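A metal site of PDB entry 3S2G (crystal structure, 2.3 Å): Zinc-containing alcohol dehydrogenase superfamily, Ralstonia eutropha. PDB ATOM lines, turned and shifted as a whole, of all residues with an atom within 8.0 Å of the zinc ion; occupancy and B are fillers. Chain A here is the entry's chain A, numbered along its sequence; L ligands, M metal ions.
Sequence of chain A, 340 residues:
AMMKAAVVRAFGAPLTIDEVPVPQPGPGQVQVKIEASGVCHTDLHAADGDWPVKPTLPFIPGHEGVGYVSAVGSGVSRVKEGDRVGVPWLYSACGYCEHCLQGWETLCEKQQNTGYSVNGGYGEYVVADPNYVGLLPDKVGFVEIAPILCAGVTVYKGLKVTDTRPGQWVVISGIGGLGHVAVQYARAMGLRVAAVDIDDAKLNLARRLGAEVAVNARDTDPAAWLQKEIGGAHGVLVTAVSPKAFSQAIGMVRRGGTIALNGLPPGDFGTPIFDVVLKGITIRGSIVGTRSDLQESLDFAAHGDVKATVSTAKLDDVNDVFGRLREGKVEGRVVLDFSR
A ring nitrogen (NE2) of His 63 lies close to an oxygen (O2) of the ligand (2.7 Å).
The side-chain sulfur (SG) of Cys 40 sits close to an oxygen (O2) of the ligand (3.5 Å).
The side-chain hydroxyl of Thr 42 lies within hydrogen-bond range of an oxygen (O2) of the ligand, at 2.7 Å.
The side-chain sulfur (SG) of Cys 150 sits close to an oxygen (O2) of the ligand (3.1 Å).
The backbone carbonyl oxygen (O) of Glu 64 lies within hydrogen-bond range of the backbone NH (N) of Gly 38 (3.0 Å).
SG of Cys 40 sits close to N of Thr 42 (3.1 Å).
The backbone carbonyl oxygen (O) of Cys 150 is in hydrogen-bond range of the side-chain hydroxyl (OG1) of Thr 154.
NH2 of Arg 333 lies within salt-bridge range of OE1 of Glu 64, at 3.4 Å.
OD2 of Asp 43 lies within hydrogen-bond range of N of Cys 40 (3.1 Å).
A ring nitrogen (ND1) of His 63 sits close to the side-chain carboxylate of Asp 43 (3.3 Å).
Of the 22 residues printed, 4 come within 4 Å of the zinc ion.
The zinc ion is bound by OE2 of Glu 64 (2.2 Å), NE2 of His 63 (2.3 Å), SG of Cys 150 (2.5 Å) and SG of Cys 40 (2.5 Å).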
ATOM      1  N   GLY A  38     -13.764  10.491   6.573  1.00  0.00           N
ATOM      2  CA  GLY A  38     -13.913   9.638   5.410  1.00  0.00           C
ATOM      3  C   GLY A  38     -12.727   9.656   4.459  1.00  0.00           C
ATOM      4  O   GLY A  38     -12.044  10.677   4.317  1.00  0.00           O
ATOM      5  N   VAL A  39     -12.482   8.519   3.826  1.00  0.00           N
ATOM      6  CA  VAL A  39     -11.390   8.373   2.863  1.00  0.00           C
ATOM      7  C   VAL A  39     -11.947   7.949   1.510  1.00  0.00           C
ATOM      8  O   VAL A  39     -12.818   7.081   1.435  1.00  0.00           O
ATOM      9  CB  VAL A  39     -10.375   7.318   3.329  1.00  0.00           C
ATOM     10  CG1 VAL A  39      -9.248   7.180   2.312  1.00  0.00           C
ATOM     11  CG2 VAL A  39      -9.828   7.668   4.705  1.00  0.00           C
ATOM     12  N   CYS A  40     -11.452   8.564   0.439  1.00  0.00           N
ATOM     13  CA  CYS A  40     -11.891   8.224  -0.905  1.00  0.00           C
ATOM     14  C   CYS A  40     -10.724   8.363  -1.899  1.00  0.00           C
ATOM     15  O   CYS A  40      -9.635   8.786  -1.532  1.00  0.00           O
ATOM     16  CB  CYS A  40     -13.036   9.136  -1.340  1.00  0.00           C
ATOM     17  SG  CYS A  40     -12.489  10.627  -2.175  1.00  0.00           S
ATOM     18  N   HIS A  41     -10.985   8.009  -3.151  1.00  0.00           N
ATOM     19  CA  HIS A  41      -9.962   8.021  -4.193  1.00  0.00           C
ATOM     20  C   HIS A  41      -9.386   9.415  -4.491  1.00  0.00           C
ATOM     21  O   HIS A  41      -8.279   9.523  -5.013  1.00  0.00           O
ATOM     22  CB  HIS A  41     -10.486   7.379  -5.481  1.00  0.00           C
ATOM     23  CG  HIS A  41     -10.373   5.885  -5.488  1.00  0.00           C
ATOM     24  ND1 HIS A  41      -9.262   5.218  -5.961  1.00  0.00           N
ATOM     25  CD2 HIS A  41     -11.235   4.925  -5.076  1.00  0.00           C
ATOM     26  CE1 HIS A  41      -9.445   3.908  -5.835  1.00  0.00           C
ATOM     27  NE2 HIS A  41     -10.638   3.706  -5.306  1.00  0.00           N
ATOM     28  N   THR A  42     -10.132  10.461  -4.165  1.00  0.00           N
ATOM     29  CA  THR A  42      -9.650  11.822  -4.342  1.00  0.00           C
ATOM     30  C   THR A  42      -8.421  12.050  -3.467  1.00  0.00           C
ATOM     31  O   THR A  42      -7.503  12.780  -3.841  1.00  0.00           O
ATOM     32  CB  THR A  42     -10.728  12.864  -3.987  1.00  0.00           C
ATOM     33  OG1 THR A  42     -11.760  12.829  -4.973  1.00  0.00           O
ATOM     34  CG2 THR A  42     -10.127  14.263  -3.933  1.00  0.00           C
ATOM     35  N   ASP A  43      -8.410  11.404  -2.308  1.00  0.00           N
ATOM     36  CA  ASP A  43      -7.285  11.492  -1.380  1.00  0.00           C
ATOM     37  C   ASP A  43      -6.024  10.876  -1.994  1.00  0.00           C
ATOM     38  O   ASP A  43      -4.916  11.321  -1.727  1.00  0.00           O
ATOM     39  CB  ASP A  43      -7.613  10.821  -0.048  1.00  0.00           C
ATOM     40  CG  ASP A  43      -8.803  11.468   0.640  1.00  0.00           C
ATOM     41  OD1 ASP A  43      -9.000  12.693   0.454  1.00  0.00           O
ATOM     42  OD2 ASP A  43      -9.522  10.765   1.377  1.00  0.00           O
ATOM     43  N   GLY A  62      -7.971  14.930   3.415  1.00  0.00           N
ATOM     44  CA  GLY A  62      -9.226  14.718   4.118  1.00  0.00           C
ATOM     45  C   GLY A  62     -10.253  15.808   3.887  1.00  0.00           C
ATOM     46  O   GLY A  62     -10.138  16.914   4.431  1.00  0.00           O
ATOM     47  N   HIS A  63     -11.275  15.494   3.105  1.00  0.00           N
ATOM     48  CA  HIS A  63     -12.369  16.415   2.846  1.00  0.00           C
ATOM     49  C   HIS A  63     -13.703  15.792   3.271  1.00  0.00           C
ATOM     50  O   HIS A  63     -14.772  16.223   2.836  1.00  0.00           O
ATOM     51  CB  HIS A  63     -12.416  16.821   1.374  1.00  0.00           C
ATOM     52  CG  HIS A  63     -12.467  15.656   0.427  1.00  0.00           C
ATOM     53  ND1 HIS A  63     -11.335  14.971   0.032  1.00  0.00           N
ATOM     54  CD2 HIS A  63     -13.501  15.054  -0.188  1.00  0.00           C
ATOM     55  CE1 HIS A  63     -11.682  13.994  -0.791  1.00  0.00           C
ATOM     56  NE2 HIS A  63     -12.994  14.026  -0.941  1.00  0.00           N
ATOM     57  N   GLU A  64     -13.617  14.780   4.130  1.00  0.00           N
ATOM     58  CA  GLU A  64     -14.804  14.133   4.677  1.00  0.00           C
ATOM     59  C   GLU A  64     -14.722  14.070   6.191  1.00  0.00           C
ATOM     60  O   GLU A  64     -15.174  13.099   6.804  1.00  0.00           O
ATOM     61  CB  GLU A  64     -14.966  12.732   4.104  1.00  0.00           C
ATOM     62  CG  GLU A  64     -14.959  12.648   2.595  1.00  0.00           C
ATOM     63  CD  GLU A  64     -15.100  11.228   2.099  1.00  0.00           C
ATOM     64  OE1 GLU A  64     -15.669  10.395   2.846  1.00  0.00           O
ATOM     65  OE2 GLU A  64     -14.643  10.918   0.979  1.00  0.00           O
ATOM     66  N   TRP A  89     -15.356  19.085   0.684  1.00  0.00           N
ATOM     67  CA  TRP A  89     -14.465  19.484  -0.407  1.00  0.00           C
ATOM     68  C   TRP A  89     -14.391  20.991  -0.604  1.00  0.00           C
ATOM     69  O   TRP A  89     -13.306  21.562  -0.697  1.00  0.00           O
ATOM     70  CB  TRP A  89     -14.925  18.818  -1.710  1.00  0.00           C
ATOM     71  CG  TRP A  89     -14.102  19.187  -2.910  1.00  0.00           C
ATOM     72  CD1 TRP A  89     -14.498  19.948  -3.983  1.00  0.00           C
ATOM     73  CD2 TRP A  89     -12.750  18.799  -3.185  1.00  0.00           C
ATOM     74  NE1 TRP A  89     -13.466  20.051  -4.887  1.00  0.00           N
ATOM     75  CE2 TRP A  89     -12.388  19.358  -4.427  1.00  0.00           C
ATOM     76  CE3 TRP A  89     -11.809  18.032  -2.487  1.00  0.00           C
ATOM     77  CZ2 TRP A  89     -11.123  19.176  -4.988  1.00  0.00           C
ATOM     78  CZ3 TRP A  89     -10.553  17.854  -3.046  1.00  0.00           C
ATOM     79  CH2 TRP A  89     -10.228  18.430  -4.289  1.00  0.00           C
ATOM     80  N   TYR A 122      -7.567  14.777   7.975  1.00  0.00           N
ATOM     81  CA  TYR A 122      -6.693  13.678   8.364  1.00  0.00           C
ATOM     82  C   TYR A 122      -5.923  14.018   9.634  1.00  0.00           C
ATOM     83  O   TYR A 122      -4.765  13.636   9.801  1.00  0.00           O
ATOM     84  CB  TYR A 122      -5.716  13.314   7.233  1.00  0.00           C
ATOM     85  CG  TYR A 122      -6.289  12.400   6.166  1.00  0.00           C
ATOM     86  CD1 TYR A 122      -5.461  11.563   5.424  1.00  0.00           C
ATOM     87  CD2 TYR A 122      -7.661  12.367   5.903  1.00  0.00           C
ATOM     88  CE1 TYR A 122      -5.973  10.736   4.448  1.00  0.00           C
ATOM     89  CE2 TYR A 122      -8.176  11.531   4.922  1.00  0.00           C
ATOM     90  CZ  TYR A 122      -7.323  10.721   4.202  1.00  0.00           C
ATOM     91  OH  TYR A 122      -7.825   9.891   3.223  1.00  0.00           O
ATOM     92  N   ALA A 146     -20.044  10.533   7.598  1.00  0.00           N
ATOM     93  CA  ALA A 146     -18.852  11.078   6.949  1.00  0.00           C
ATOM     94  C   ALA A 146     -18.868  11.004   5.413  1.00  0.00           C
ATOM     95  O   ALA A 146     -18.616  11.995   4.745  1.00  0.00           O
ATOM     96  CB  ALA A 146     -17.582  10.430   7.517  1.00  0.00           C
ATOM     97  N   PRO A 147     -19.147   9.815   4.853  1.00  0.00           N
ATOM     98  CA  PRO A 147     -19.121   9.629   3.397  1.00  0.00           C
ATOM     99  C   PRO A 147     -20.155  10.470   2.649  1.00  0.00           C
ATOM    100  O   PRO A 147     -20.006  10.687   1.443  1.00  0.00           O
ATOM    101  CB  PRO A 147     -19.443   8.144   3.222  1.00  0.00           C
ATOM    102  CG  PRO A 147     -19.058   7.517   4.521  1.00  0.00           C
ATOM    103  CD  PRO A 147     -19.384   8.543   5.559  1.00  0.00           C
ATOM    104  N   LEU A 149     -20.611  13.540   2.964  1.00  0.00           N
ATOM    105  CA  LEU A 149     -19.966  14.804   2.648  1.00  0.00           C
ATOM    106  C   LEU A 149     -19.372  14.810   1.244  1.00  0.00           C
ATOM    107  O   LEU A 149     -19.115  15.870   0.683  1.00  0.00           O
ATOM    108  CB  LEU A 149     -18.854  15.112   3.653  1.00  0.00           C
ATOM    109  CG  LEU A 149     -19.263  15.462   5.074  1.00  0.00           C
ATOM    110  CD1 LEU A 149     -18.022  15.708   5.923  1.00  0.00           C
ATOM    111  CD2 LEU A 149     -20.170  16.684   5.071  1.00  0.00           C
ATOM    112  N   CYS A 150     -19.148  13.622   0.699  1.00  0.00           N
ATOM    113  CA  CYS A 150     -18.529  13.519  -0.613  1.00  0.00           C
ATOM    114  C   CYS A 150     -19.329  12.614  -1.541  1.00  0.00           C
ATOM    115  O   CYS A 150     -19.945  13.081  -2.492  1.00  0.00           O
ATOM    116  CB  CYS A 150     -17.098  12.984  -0.486  1.00  0.00           C
ATOM    117  SG  CYS A 150     -16.342  12.578  -2.062  1.00  0.00           S
ATOM    118  N   ALA A 151     -19.293  11.309  -1.272  1.00  0.00           N
ATOM    119  CA  ALA A 151     -20.041  10.347  -2.065  1.00  0.00           C
ATOM    120  C   ALA A 151     -21.526  10.701  -2.094  1.00  0.00           C
ATOM    121  O   ALA A 151     -22.154  10.655  -3.153  1.00  0.00           O
ATOM    122  CB  ALA A 151     -19.839   8.949  -1.529  1.00  0.00           C
ATOM    123  N   GLY A 152     -22.066  11.057  -0.937  1.00  0.00           N
ATOM    124  CA  GLY A 152     -23.477  11.371  -0.812  1.00  0.00           C
ATOM    125  C   GLY A 152     -23.938  12.511  -1.712  1.00  0.00           C
ATOM    126  O   GLY A 152     -24.722  12.312  -2.633  1.00  0.00           O
ATOM    127  N   THR A 154     -22.381  14.072  -3.990  1.00  0.00           N
ATOM    128  CA  THR A 154     -21.969  13.857  -5.372  1.00  0.00           C
ATOM    129  C   THR A 154     -23.035  13.143  -6.189  1.00  0.00           C
ATOM    130  O   THR A 154     -23.448  13.631  -7.241  1.00  0.00           O
ATOM    131  CB  THR A 154     -20.656  13.063  -5.454  1.00  0.00           C
ATOM    132  OG1 THR A 154     -19.564  13.929  -5.108  1.00  0.00           O
ATOM    133  CG2 THR A 154     -20.441  12.521  -6.851  1.00  0.00           C
ATOM    134  N   LEU A 178     -19.502   5.014  -4.825  1.00  0.00           N
ATOM    135  CA  LEU A 178     -20.509   6.011  -5.164  1.00  0.00           C
ATOM    136  C   LEU A 178     -21.833   5.331  -5.534  1.00  0.00           C
ATOM    137  O   LEU A 178     -22.891   5.703  -5.031  1.00  0.00           O
ATOM    138  CB  LEU A 178     -20.046   6.874  -6.341  1.00  0.00           C
ATOM    139  CG  LEU A 178     -18.800   7.745  -6.145  1.00  0.00           C
ATOM    140  CD1 LEU A 178     -18.577   8.624  -7.356  1.00  0.00           C
ATOM    141  CD2 LEU A 178     -18.950   8.593  -4.901  1.00  0.00           C
ATOM    142  N   ILE A 287     -19.813  16.800  -9.898  1.00  0.00           N
ATOM    143  CA  ILE A 287     -19.134  16.227  -8.735  1.00  0.00           C
ATOM    144  C   ILE A 287     -19.389  17.099  -7.518  1.00  0.00           C
ATOM    145  O   ILE A 287     -19.553  18.318  -7.642  1.00  0.00           O
ATOM    146  CB  ILE A 287     -17.611  16.054  -8.979  1.00  0.00           C
ATOM    147  CG1 ILE A 287     -16.970  15.289  -7.823  1.00  0.00           C
ATOM    148  CG2 ILE A 287     -16.931  17.407  -9.181  1.00  0.00           C
ATOM    149  CD1 ILE A 287     -15.560  14.844  -8.083  1.00  0.00           C
ATOM    150  N   VAL A 288     -19.425  16.485  -6.331  1.00  0.00           N
ATOM    151  CA  VAL A 288     -19.895  17.146  -5.108  1.00  0.00           C
ATOM    152  C   VAL A 288     -21.112  18.031  -5.375  1.00  0.00           C
ATOM    153  O   VAL A 288     -21.901  17.746  -6.279  1.00  0.00           O
ATOM    154  CB  VAL A 288     -18.777  17.952  -4.396  1.00  0.00           C
ATOM    155  CG1 VAL A 288     -17.665  17.020  -3.934  1.00  0.00           C
ATOM    156  CG2 VAL A 288     -18.229  19.054  -5.284  1.00  0.00           C
ATOM    157  N   ARG A 333     -17.208   2.213   1.653  1.00  0.00           N
ATOM    158  CA  ARG A 333     -16.293   3.302   1.966  1.00  0.00           C
ATOM    159  C   ARG A 333     -15.532   3.059   3.261  1.00  0.00           C
ATOM    160  O   ARG A 333     -16.063   2.458   4.197  1.00  0.00           O
ATOM    161  CB  ARG A 333     -17.041   4.631   2.068  1.00  0.00           C
ATOM    162  CG  ARG A 333     -17.316   5.317   0.734  1.00  0.00           C
ATOM    163  CD  ARG A 333     -16.044   5.898   0.140  1.00  0.00           C
ATOM    164  NE  ARG A 333     -16.317   6.645  -1.089  1.00  0.00           N
ATOM    165  CZ  ARG A 333     -16.439   7.970  -1.147  1.00  0.00           C
ATOM    166  NH1 ARG A 333     -16.689   8.563  -2.315  1.00  0.00           N
ATOM    167  NH2 ARG A 333     -16.327   8.705  -0.056  1.00  0.00           N
HETATM  168  C1  LIG L   1     -14.450  14.842  -3.716  1.00  0.00           C
HETATM  169  C2  LIG L   1     -13.996  15.663  -4.868  1.00  0.00           C
HETATM  170  O1  LIG L   1     -12.894  15.406  -5.607  1.00  0.00           O
HETATM  171  C3  LIG L   1     -12.755  16.331  -6.584  1.00  0.00           C
HETATM  172  C4  LIG L   1     -13.815  17.211  -6.478  1.00  0.00           C
HETATM  173  C5  LIG L   1     -14.597  16.793  -5.401  1.00  0.00           C
HETATM  174  O2  LIG L   1     -13.796  13.651  -3.487  1.00  0.00           O
HETATM  175 ZN    ZN M   1     -14.163  12.046  -0.903  1.00  0.00          ZN
